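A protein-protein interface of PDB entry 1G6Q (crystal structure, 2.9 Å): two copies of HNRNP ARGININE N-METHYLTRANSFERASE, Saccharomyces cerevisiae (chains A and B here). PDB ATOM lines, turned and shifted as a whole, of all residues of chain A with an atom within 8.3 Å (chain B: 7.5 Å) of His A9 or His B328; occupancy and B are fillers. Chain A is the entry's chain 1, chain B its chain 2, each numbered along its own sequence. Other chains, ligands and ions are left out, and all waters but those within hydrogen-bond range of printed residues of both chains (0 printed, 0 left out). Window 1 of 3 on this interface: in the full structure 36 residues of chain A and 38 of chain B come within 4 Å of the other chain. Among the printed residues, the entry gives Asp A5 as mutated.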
ATOM      1  N   PHE A   4       8.401 -36.906  -2.270  1.00  0.00           N
ATOM      2  CA  PHE A   4       8.549 -36.436  -3.629  1.00  0.00           C
ATOM      3  C   PHE A   4       9.189 -37.363  -4.670  1.00  0.00           C
ATOM      4  O   PHE A   4      10.390 -37.438  -4.936  1.00  0.00           O
ATOM      5  CB  PHE A   4       9.270 -35.112  -3.519  1.00  0.00           C
ATOM      6  CG  PHE A   4       8.272 -34.065  -3.077  1.00  0.00           C
ATOM      7  CD1 PHE A   4       7.283 -33.638  -3.988  1.00  0.00           C
ATOM      8  CD2 PHE A   4       8.307 -33.564  -1.772  1.00  0.00           C
ATOM      9  CE1 PHE A   4       6.321 -32.706  -3.588  1.00  0.00           C
ATOM     10  CE2 PHE A   4       7.341 -32.637  -1.382  1.00  0.00           C
ATOM     11  CZ  PHE A   4       6.365 -32.221  -2.286  1.00  0.00           C
ATOM     12  N   ASP A   5       8.284 -38.130  -5.258  1.00  0.00           N
ATOM     13  CA  ASP A   5       8.635 -39.082  -6.313  1.00  0.00           C
ATOM     14  C   ASP A   5       8.468 -38.582  -7.764  1.00  0.00           C
ATOM     15  O   ASP A   5       8.760 -39.272  -8.741  1.00  0.00           O
ATOM     16  CB  ASP A   5       7.787 -40.378  -6.079  1.00  0.00           C
ATOM     17  CG  ASP A   5       6.256 -40.277  -6.173  1.00  0.00           C
ATOM     18  OD1 ASP A   5       5.681 -40.911  -7.055  1.00  0.00           O
ATOM     19  OD2 ASP A   5       5.629 -39.592  -5.362  1.00  0.00           O
ATOM     20  N   SER A   6       7.997 -37.351  -7.959  1.00  0.00           N
ATOM     21  CA  SER A   6       7.620 -36.818  -9.282  1.00  0.00           C
ATOM     22  C   SER A   6       8.239 -35.513  -9.804  1.00  0.00           C
ATOM     23  O   SER A   6       8.415 -34.563  -9.039  1.00  0.00           O
ATOM     24  CB  SER A   6       6.095 -36.660  -9.296  1.00  0.00           C
ATOM     25  OG  SER A   6       5.602 -35.902  -8.181  1.00  0.00           O
ATOM     26  N   TYR A   7       8.579 -35.374 -11.096  1.00  0.00           N
ATOM     27  CA  TYR A   7       9.131 -34.119 -11.616  1.00  0.00           C
ATOM     28  C   TYR A   7       8.160 -32.962 -11.654  1.00  0.00           C
ATOM     29  O   TYR A   7       8.483 -31.826 -11.360  1.00  0.00           O
ATOM     30  CB  TYR A   7       9.677 -34.253 -13.066  1.00  0.00           C
ATOM     31  CG  TYR A   7       9.709 -32.961 -13.909  1.00  0.00           C
ATOM     32  CD1 TYR A   7       8.739 -32.683 -14.889  1.00  0.00           C
ATOM     33  CD2 TYR A   7      10.737 -32.040 -13.681  1.00  0.00           C
ATOM     34  CE1 TYR A   7       8.798 -31.501 -15.632  1.00  0.00           C
ATOM     35  CE2 TYR A   7      10.802 -30.854 -14.425  1.00  0.00           C
ATOM     36  CZ  TYR A   7       9.826 -30.595 -15.391  1.00  0.00           C
ATOM     37  OH  TYR A   7       9.850 -29.404 -16.084  1.00  0.00           O
ATOM     38  N   ASP A   8       7.040 -33.199 -12.285  1.00  0.00           N
ATOM     39  CA  ASP A   8       6.043 -32.160 -12.528  1.00  0.00           C
ATOM     40  C   ASP A   8       6.029 -30.703 -12.027  1.00  0.00           C
ATOM     41  O   ASP A   8       5.705 -30.200 -10.947  1.00  0.00           O
ATOM     42  CB  ASP A   8       4.713 -32.768 -12.188  1.00  0.00           C
ATOM     43  CG  ASP A   8       4.802 -33.649 -10.967  1.00  0.00           C
ATOM     44  OD1 ASP A   8       4.369 -34.793 -11.102  1.00  0.00           O
ATOM     45  OD2 ASP A   8       5.326 -33.199  -9.934  1.00  0.00           O
ATOM     46  N   HIS A   9       6.526 -30.028 -13.032  1.00  0.00           N
ATOM     47  CA  HIS A   9       6.442 -28.600 -13.100  1.00  0.00           C
ATOM     48  C   HIS A   9       5.035 -28.274 -13.589  1.00  0.00           C
ATOM     49  O   HIS A   9       4.902 -28.019 -14.793  1.00  0.00           O
ATOM     50  CB  HIS A   9       7.425 -28.157 -14.095  1.00  0.00           C
ATOM     51  CG  HIS A   9       8.649 -27.626 -13.458  1.00  0.00           C
ATOM     52  ND1 HIS A   9       9.893 -27.785 -13.855  1.00  0.00           N
ATOM     53  CD2 HIS A   9       8.627 -26.750 -12.414  1.00  0.00           C
ATOM     54  CE1 HIS A   9      10.644 -27.023 -13.102  1.00  0.00           C
ATOM     55  NE2 HIS A   9       9.866 -26.414 -12.244  1.00  0.00           N
ATOM     56  N   TYR A  10       3.964 -28.229 -12.777  1.00  0.00           N
ATOM     57  CA  TYR A  10       2.620 -28.000 -13.325  1.00  0.00           C
ATOM     58  C   TYR A  10       2.478 -26.818 -14.287  1.00  0.00           C
ATOM     59  O   TYR A  10       1.890 -26.976 -15.361  1.00  0.00           O
ATOM     60  CB  TYR A  10       1.593 -27.839 -12.190  1.00  0.00           C
ATOM     61  CG  TYR A  10       1.451 -26.447 -11.615  1.00  0.00           C
ATOM     62  CD1 TYR A  10       2.361 -26.008 -10.673  1.00  0.00           C
ATOM     63  CD2 TYR A  10       0.422 -25.617 -12.067  1.00  0.00           C
ATOM     64  CE1 TYR A  10       2.248 -24.709 -10.181  1.00  0.00           C
ATOM     65  CE2 TYR A  10       0.311 -24.319 -11.578  1.00  0.00           C
ATOM     66  CZ  TYR A  10       1.226 -23.884 -10.634  1.00  0.00           C
ATOM     67  OH  TYR A  10       1.126 -22.613 -10.135  1.00  0.00           O
ATOM     68  N   GLY A  11       3.126 -25.692 -13.957  1.00  0.00           N
ATOM     69  CA  GLY A  11       3.138 -24.491 -14.790  1.00  0.00           C
ATOM     70  C   GLY A  11       3.232 -24.722 -16.304  1.00  0.00           C
ATOM     71  O   GLY A  11       2.378 -24.232 -17.052  1.00  0.00           O
ATOM     72  N   ILE A  12       4.159 -25.547 -16.802  1.00  0.00           N
ATOM     73  CA  ILE A  12       4.263 -25.714 -18.259  1.00  0.00           C
ATOM     74  C   ILE A  12       3.101 -26.448 -18.950  1.00  0.00           C
ATOM     75  O   ILE A  12       2.754 -26.238 -20.109  1.00  0.00           O
ATOM     76  CB  ILE A  12       5.608 -26.416 -18.586  1.00  0.00           C
ATOM     77  CG1 ILE A  12       5.788 -26.416 -20.104  1.00  0.00           C
ATOM     78  CG2 ILE A  12       5.644 -27.804 -17.980  1.00  0.00           C
ATOM     79  CD1 ILE A  12       7.106 -27.007 -20.643  1.00  0.00           C
ATOM     80  N   HIS A  13       2.434 -27.312 -18.201  1.00  0.00           N
ATOM     81  CA  HIS A  13       1.266 -27.991 -18.732  1.00  0.00           C
ATOM     82  C   HIS A  13       0.028 -27.112 -18.641  1.00  0.00           C
ATOM     83  O   HIS A  13      -0.884 -27.173 -19.463  1.00  0.00           O
ATOM     84  CB  HIS A  13       1.061 -29.305 -17.979  1.00  0.00           C
ATOM     85  CG  HIS A  13       2.072 -30.311 -18.521  1.00  0.00           C
ATOM     86  ND1 HIS A  13       3.204 -30.784 -18.009  1.00  0.00           N
ATOM     87  CD2 HIS A  13       1.941 -30.844 -19.781  1.00  0.00           C
ATOM     88  CE1 HIS A  13       3.753 -31.562 -18.905  1.00  0.00           C
ATOM     89  NE2 HIS A  13       2.990 -31.592 -19.961  1.00  0.00           N
ATOM     90  N   GLU A  14      -0.001 -26.238 -17.640  1.00  0.00           N
ATOM     91  CA  GLU A  14      -1.060 -25.237 -17.506  1.00  0.00           C
ATOM     92  C   GLU A  14      -0.975 -24.300 -18.719  1.00  0.00           C
ATOM     93  O   GLU A  14      -1.989 -24.011 -19.341  1.00  0.00           O
ATOM     94  CB  GLU A  14      -0.845 -24.459 -16.209  1.00  0.00           C
ATOM     95  CG  GLU A  14      -1.864 -23.329 -15.993  1.00  0.00           C
ATOM     96  CD  GLU A  14      -1.628 -22.413 -14.799  1.00  0.00           C
ATOM     97  OE1 GLU A  14      -2.550 -22.258 -14.005  1.00  0.00           O
ATOM     98  OE2 GLU A  14      -0.543 -21.839 -14.676  1.00  0.00           O
ATOM     99  N   GLU A  15       0.234 -23.862 -19.079  1.00  0.00           N
ATOM    100  CA  GLU A  15       0.458 -23.043 -20.263  1.00  0.00           C
ATOM    101  C   GLU A  15      -0.024 -23.737 -21.544  1.00  0.00           C
ATOM    102  O   GLU A  15      -0.735 -23.152 -22.362  1.00  0.00           O
ATOM    103  CB  GLU A  15       1.957 -22.730 -20.339  1.00  0.00           C
ATOM    104  CG  GLU A  15       2.421 -21.750 -21.432  1.00  0.00           C
ATOM    105  CD  GLU A  15       3.936 -21.553 -21.494  1.00  0.00           C
ATOM    106  OE1 GLU A  15       4.381 -20.415 -21.370  1.00  0.00           O
ATOM    107  OE2 GLU A  15       4.668 -22.526 -21.676  1.00  0.00           O
ATOM    108  N   SER A  70       8.480 -37.737 -20.336  1.00  0.00           N
ATOM    109  CA  SER A  70       8.422 -36.944 -19.104  1.00  0.00           C
ATOM    110  C   SER A  70       7.574 -37.517 -17.992  1.00  0.00           C
ATOM    111  O   SER A  70       6.500 -38.047 -18.277  1.00  0.00           O
ATOM    112  CB  SER A  70       7.882 -35.571 -19.398  1.00  0.00           C
ATOM    113  OG  SER A  70       7.298 -34.906 -18.284  1.00  0.00           O
ATOM    114  N   SER A  71       7.970 -37.351 -16.719  1.00  0.00           N
ATOM    115  CA  SER A  71       7.234 -37.864 -15.535  1.00  0.00           C
ATOM    116  C   SER A  71       5.725 -37.636 -15.444  1.00  0.00           C
ATOM    117  O   SER A  71       4.976 -38.334 -14.758  1.00  0.00           O
ATOM    118  CB  SER A  71       7.786 -37.303 -14.222  1.00  0.00           C
ATOM    119  OG  SER A  71       7.390 -35.963 -13.935  1.00  0.00           O
ATOM    120  N   ILE A  72       5.253 -36.612 -16.157  1.00  0.00           N
ATOM    121  CA  ILE A  72       3.832 -36.319 -16.266  1.00  0.00           C
ATOM    122  C   ILE A  72       2.989 -37.520 -16.743  1.00  0.00           C
ATOM    123  O   ILE A  72       1.783 -37.517 -16.522  1.00  0.00           O
ATOM    124  CB  ILE A  72       3.701 -35.083 -17.198  1.00  0.00           C
ATOM    125  CG1 ILE A  72       2.425 -34.381 -16.897  1.00  0.00           C
ATOM    126  CG2 ILE A  72       3.689 -35.477 -18.658  1.00  0.00           C
ATOM    127  CD1 ILE A  72       2.482 -33.735 -15.509  1.00  0.00           C
ATOM    128  N   TYR B 120      18.295 -21.942  -3.403  1.00  0.00           N
ATOM    129  CA  TYR B 120      17.843 -22.816  -4.477  1.00  0.00           C
ATOM    130  C   TYR B 120      18.851 -23.142  -5.560  1.00  0.00           C
ATOM    131  O   TYR B 120      19.510 -24.143  -5.316  1.00  0.00           O
ATOM    132  CB  TYR B 120      16.577 -22.280  -5.135  1.00  0.00           C
ATOM    133  CG  TYR B 120      16.078 -23.178  -6.249  1.00  0.00           C
ATOM    134  CD1 TYR B 120      15.963 -22.651  -7.518  1.00  0.00           C
ATOM    135  CD2 TYR B 120      15.848 -24.530  -6.054  1.00  0.00           C
ATOM    136  CE1 TYR B 120      15.646 -23.470  -8.600  1.00  0.00           C
ATOM    137  CE2 TYR B 120      15.532 -25.368  -7.120  1.00  0.00           C
ATOM    138  CZ  TYR B 120      15.439 -24.832  -8.392  1.00  0.00           C
ATOM    139  OH  TYR B 120      15.216 -25.652  -9.485  1.00  0.00           O
ATOM    140  N   GLU B 121      19.114 -22.576  -6.735  1.00  0.00           N
ATOM    141  CA  GLU B 121      20.224 -23.177  -7.495  1.00  0.00           C
ATOM    142  C   GLU B 121      21.461 -22.344  -7.334  1.00  0.00           C
ATOM    143  O   GLU B 121      21.981 -21.673  -8.224  1.00  0.00           O
ATOM    144  CB  GLU B 121      19.854 -23.314  -8.920  1.00  0.00           C
ATOM    145  CG  GLU B 121      19.065 -24.596  -8.994  1.00  0.00           C
ATOM    146  CD  GLU B 121      18.655 -25.035 -10.382  1.00  0.00           C
ATOM    147  OE1 GLU B 121      17.995 -24.274 -11.096  1.00  0.00           O
ATOM    148  OE2 GLU B 121      18.996 -26.167 -10.729  1.00  0.00           O
ATOM    149  N   PHE B 177      -4.439 -32.388 -10.207  1.00  0.00           N
ATOM    150  CA  PHE B 177      -3.538 -31.263 -10.274  1.00  0.00           C
ATOM    151  C   PHE B 177      -3.641 -30.306  -9.086  1.00  0.00           C
ATOM    152  O   PHE B 177      -2.653 -29.645  -8.749  1.00  0.00           O
ATOM    153  CB  PHE B 177      -3.804 -30.476 -11.510  1.00  0.00           C
ATOM    154  CG  PHE B 177      -2.957 -30.950 -12.654  1.00  0.00           C
ATOM    155  CD1 PHE B 177      -3.332 -32.040 -13.420  1.00  0.00           C
ATOM    156  CD2 PHE B 177      -1.765 -30.285 -12.928  1.00  0.00           C
ATOM    157  CE1 PHE B 177      -2.501 -32.453 -14.464  1.00  0.00           C
ATOM    158  CE2 PHE B 177      -0.947 -30.709 -13.976  1.00  0.00           C
ATOM    159  CZ  PHE B 177      -1.312 -31.794 -14.754  1.00  0.00           C
ATOM    160  N   LEU B 180      -0.909 -30.819  -6.537  1.00  0.00           N
ATOM    161  CA  LEU B 180       0.320 -30.537  -7.244  1.00  0.00           C
ATOM    162  C   LEU B 180       0.594 -29.055  -7.248  1.00  0.00           C
ATOM    163  O   LEU B 180       1.666 -28.636  -6.835  1.00  0.00           O
ATOM    164  CB  LEU B 180       0.209 -31.034  -8.651  1.00  0.00           C
ATOM    165  CG  LEU B 180       1.512 -31.402  -9.349  1.00  0.00           C
ATOM    166  CD1 LEU B 180       2.108 -32.647  -8.715  1.00  0.00           C
ATOM    167  CD2 LEU B 180       1.234 -31.709 -10.802  1.00  0.00           C
ATOM    168  N   HIS B 183       1.774 -27.895  -3.897  1.00  0.00           N
ATOM    169  CA  HIS B 183       3.123 -28.319  -3.576  1.00  0.00           C
ATOM    170  C   HIS B 183       4.228 -27.578  -4.298  1.00  0.00           C
ATOM    171  O   HIS B 183       5.416 -27.908  -4.132  1.00  0.00           O
ATOM    172  CB  HIS B 183       3.314 -29.776  -3.892  1.00  0.00           C
ATOM    173  CG  HIS B 183       2.539 -30.733  -3.000  1.00  0.00           C
ATOM    174  ND1 HIS B 183       1.939 -30.485  -1.829  1.00  0.00           N
ATOM    175  CD2 HIS B 183       2.333 -32.070  -3.300  1.00  0.00           C
ATOM    176  CE1 HIS B 183       1.388 -31.608  -1.417  1.00  0.00           C
ATOM    177  NE2 HIS B 183       1.630 -32.549  -2.306  1.00  0.00           N
ATOM    178  N   GLU B 184       3.853 -26.603  -5.108  1.00  0.00           N
ATOM    179  CA  GLU B 184       4.849 -25.904  -5.876  1.00  0.00           C
ATOM    180  C   GLU B 184       5.184 -24.510  -5.381  1.00  0.00           C
ATOM    181  O   GLU B 184       4.293 -23.675  -5.239  1.00  0.00           O
ATOM    182  CB  GLU B 184       4.385 -25.837  -7.326  1.00  0.00           C
ATOM    183  CG  GLU B 184       5.488 -25.396  -8.271  1.00  0.00           C
ATOM    184  CD  GLU B 184       6.434 -26.498  -8.707  1.00  0.00           C
ATOM    185  OE1 GLU B 184       6.750 -26.507  -9.895  1.00  0.00           O
ATOM    186  OE2 GLU B 184       6.889 -27.308  -7.898  1.00  0.00           O
ATOM    187  N   PRO B 185       6.418 -24.180  -5.028  1.00  0.00           N
ATOM    188  CA  PRO B 185       6.763 -22.848  -4.595  1.00  0.00           C
ATOM    189  C   PRO B 185       6.726 -21.944  -5.823  1.00  0.00           C
ATOM    190  O   PRO B 185       7.166 -22.332  -6.916  1.00  0.00           O
ATOM    191  CB  PRO B 185       8.132 -22.934  -4.029  1.00  0.00           C
ATOM    192  CG  PRO B 185       8.602 -24.345  -4.182  1.00  0.00           C
ATOM    193  CD  PRO B 185       7.500 -25.126  -4.840  1.00  0.00           C
ATOM    194  N   ASN B 295      18.121 -36.029  -5.456  1.00  0.00           N
ATOM    195  CA  ASN B 295      18.891 -35.003  -6.158  1.00  0.00           C
ATOM    196  C   ASN B 295      19.268 -33.800  -5.273  1.00  0.00           C
ATOM    197  O   ASN B 295      18.443 -32.930  -4.991  1.00  0.00           O
ATOM    198  CB  ASN B 295      18.073 -34.550  -7.361  1.00  0.00           C
ATOM    199  CG  ASN B 295      18.817 -33.638  -8.324  1.00  0.00           C
ATOM    200  OD1 ASN B 295      19.568 -32.736  -7.988  1.00  0.00           O
ATOM    201  ND2 ASN B 295      18.650 -33.777  -9.610  1.00  0.00           N
ATOM    202  N   ARG B 297      20.531 -31.035  -5.953  1.00  0.00           N
ATOM    203  CA  ARG B 297      20.306 -29.711  -6.521  1.00  0.00           C
ATOM    204  C   ARG B 297      18.840 -29.240  -6.586  1.00  0.00           C
ATOM    205  O   ARG B 297      18.440 -28.247  -7.194  1.00  0.00           O
ATOM    206  CB  ARG B 297      20.942 -29.674  -7.884  1.00  0.00           C
ATOM    207  CG  ARG B 297      21.396 -28.239  -7.931  1.00  0.00           C
ATOM    208  CD  ARG B 297      22.291 -27.898  -9.084  1.00  0.00           C
ATOM    209  NE  ARG B 297      22.683 -26.503  -8.972  1.00  0.00           N
ATOM    210  CZ  ARG B 297      23.564 -26.066  -8.059  1.00  0.00           C
ATOM    211  NH1 ARG B 297      24.154 -26.872  -7.164  1.00  0.00           N
ATOM    212  NH2 ARG B 297      23.864 -24.774  -8.059  1.00  0.00           N
ATOM    213  N   ASP B 298      18.012 -30.045  -5.931  1.00  0.00           N
ATOM    214  CA  ASP B 298      16.614 -29.748  -5.685  1.00  0.00           C
ATOM    215  C   ASP B 298      16.464 -29.610  -4.184  1.00  0.00           C
ATOM    216  O   ASP B 298      17.182 -30.186  -3.374  1.00  0.00           O
ATOM    217  CB  ASP B 298      15.654 -30.855  -6.061  1.00  0.00           C
ATOM    218  CG  ASP B 298      15.599 -31.319  -7.518  1.00  0.00           C
ATOM    219  OD1 ASP B 298      14.891 -32.293  -7.759  1.00  0.00           O
ATOM    220  OD2 ASP B 298      16.180 -30.706  -8.425  1.00  0.00           O
ATOM    221  N   LEU B 299      15.446 -28.876  -3.777  1.00  0.00           N
ATOM    222  CA  LEU B 299      15.156 -28.656  -2.365  1.00  0.00           C
ATOM    223  C   LEU B 299      13.841 -29.171  -1.807  1.00  0.00           C
ATOM    224  O   LEU B 299      12.785 -28.887  -2.348  1.00  0.00           O
ATOM    225  CB  LEU B 299      15.197 -27.189  -2.043  1.00  0.00           C
ATOM    226  CG  LEU B 299      16.540 -26.568  -2.011  1.00  0.00           C
ATOM    227  CD1 LEU B 299      16.335 -25.130  -1.699  1.00  0.00           C
ATOM    228  CD2 LEU B 299      17.410 -27.216  -0.970  1.00  0.00           C
ATOM    229  N   LEU B 326       8.244 -29.063  -2.990  1.00  0.00           N
ATOM    230  CA  LEU B 326       9.457 -29.502  -3.692  1.00  0.00           C
ATOM    231  C   LEU B 326       9.907 -28.438  -4.658  1.00  0.00           C
ATOM    232  O   LEU B 326       9.149 -27.997  -5.518  1.00  0.00           O
ATOM    233  CB  LEU B 326       9.231 -30.755  -4.500  1.00  0.00           C
ATOM    234  CG  LEU B 326      10.379 -31.221  -5.356  1.00  0.00           C
ATOM    235  CD1 LEU B 326      11.522 -31.612  -4.440  1.00  0.00           C
ATOM    236  CD2 LEU B 326       9.928 -32.349  -6.265  1.00  0.00           C
ATOM    237  N   MET B 327      11.143 -28.034  -4.582  1.00  0.00           N
ATOM    238  CA  MET B 327      11.609 -26.963  -5.432  1.00  0.00           C
ATOM    239  C   MET B 327      12.601 -27.508  -6.447  1.00  0.00           C
ATOM    240  O   MET B 327      13.576 -28.151  -6.065  1.00  0.00           O
ATOM    241  CB  MET B 327      12.233 -25.898  -4.541  1.00  0.00           C
ATOM    242  CG  MET B 327      12.014 -24.487  -5.025  1.00  0.00           C
ATOM    243  SD  MET B 327      12.463 -23.228  -3.796  1.00  0.00           S
ATOM    244  CE  MET B 327      12.756 -22.022  -5.067  1.00  0.00           C
ATOM    245  N   HIS B 328      12.391 -27.272  -7.737  1.00  0.00           N
ATOM    246  CA  HIS B 328      13.192 -27.846  -8.832  1.00  0.00           C
ATOM    247  C   HIS B 328      12.728 -27.299 -10.195  1.00  0.00           C
ATOM    248  O   HIS B 328      11.644 -26.705 -10.250  1.00  0.00           O
ATOM    249  CB  HIS B 328      13.055 -29.356  -8.879  1.00  0.00           C
ATOM    250  CG  HIS B 328      11.610 -29.726  -9.129  1.00  0.00           C
ATOM    251  ND1 HIS B 328      10.555 -28.920  -9.017  1.00  0.00           N
ATOM    252  CD2 HIS B 328      11.146 -30.929  -9.525  1.00  0.00           C
ATOM    253  CE1 HIS B 328       9.485 -29.555  -9.314  1.00  0.00           C
ATOM    254  NE2 HIS B 328       9.867 -30.749  -9.608  1.00  0.00           N
ATOM    255  OXT HIS B 328      13.407 -27.509 -11.196  1.00  0.00           O
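No position is printed for both chains. Of the 8 pairs that touch across the chains among the printed residues, none has its exchanged pair printed and touching as well.
Of the printed residues of chain B, His A9 touches Glu B184 (3.2 Å) and His B328 (2.7 Å). His B328 touches just these residues of chain A: Tyr A7 (2.5 Å) and His A9 (2.7 Å). Printed residues of chain B within 4 Å of Phe A4: Leu B326 (3.5 Å). Printed residues of chain B within 4 Å of Asp A8: Leu B180 and Glu B184. Glu A15 touches none of the printed residues of chain B. Ser A70 touches none of the printed residues of chain B. The nearest residue of chain B that does not touch His A9 is Leu B180 (5.8 Å). The nearest printed residue of chain A that does not touch Leu B180 is Tyr A10 (4.1 Å).
Hydrophobic or aromatic side chains of chain A within 4 Å of the printed part of chain B: Phe A4, His A9 and Tyr A10. Hydrophobic or aromatic side chains of chain B within 4 Å of the printed part of chain A: Leu B180, Leu B326 and His B328. Among the printed residues, 8 pairs touch across the chains. Among the printed residues, no Asp or Glu carboxylate lies within 4 Å of a Lys or Arg side-chain nitrogen of the other chain.
The backbone carbonyl oxygen (O) of His B183 lies within hydrogen-bond range of the backbone NH (N) of Leu B326. OXT of His B328 sits close to OH of Tyr B120, 3.1 Å away. The backbone NH (N) of Asp A8 lies within hydrogen-bond range of the side-chain hydroxyl (OG) of Ser A71 (3.2 Å). The side-chain hydroxyl (OH) of Tyr A7 sits at hydrogen-bond distance from a ring nitrogen (ND1) of His A9, at 2.8 Å. N of Tyr A7 lies close to OG of Ser A71, 3.1 Å away. OG of Ser A6 lies within hydrogen-bond range of OD2 of Asp A8, at 3.2 Å.
A ring nitrogen (NE2) of His B328 lies within hydrogen-bond range of the backbone carbonyl oxygen (O) of Tyr A7. The chain-end carboxylate of His B328 is in hydrogen-bond range of a ring nitrogen (NE2) of His A9 (2.7 Å).
Phe A4 touches Leu B326 (CD1 to CB, 3.5 Å). CD2 of Leu B326 touches O of Ser A6 (3.9 Å). Asp A8 touches Leu B180. O of Asp A8 touches OE1 of Glu B184, at 3.98 Å. OE1 of Glu B184 touches CD2 of His A9 (3.2 Å). Glu B184 touches Tyr A10.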
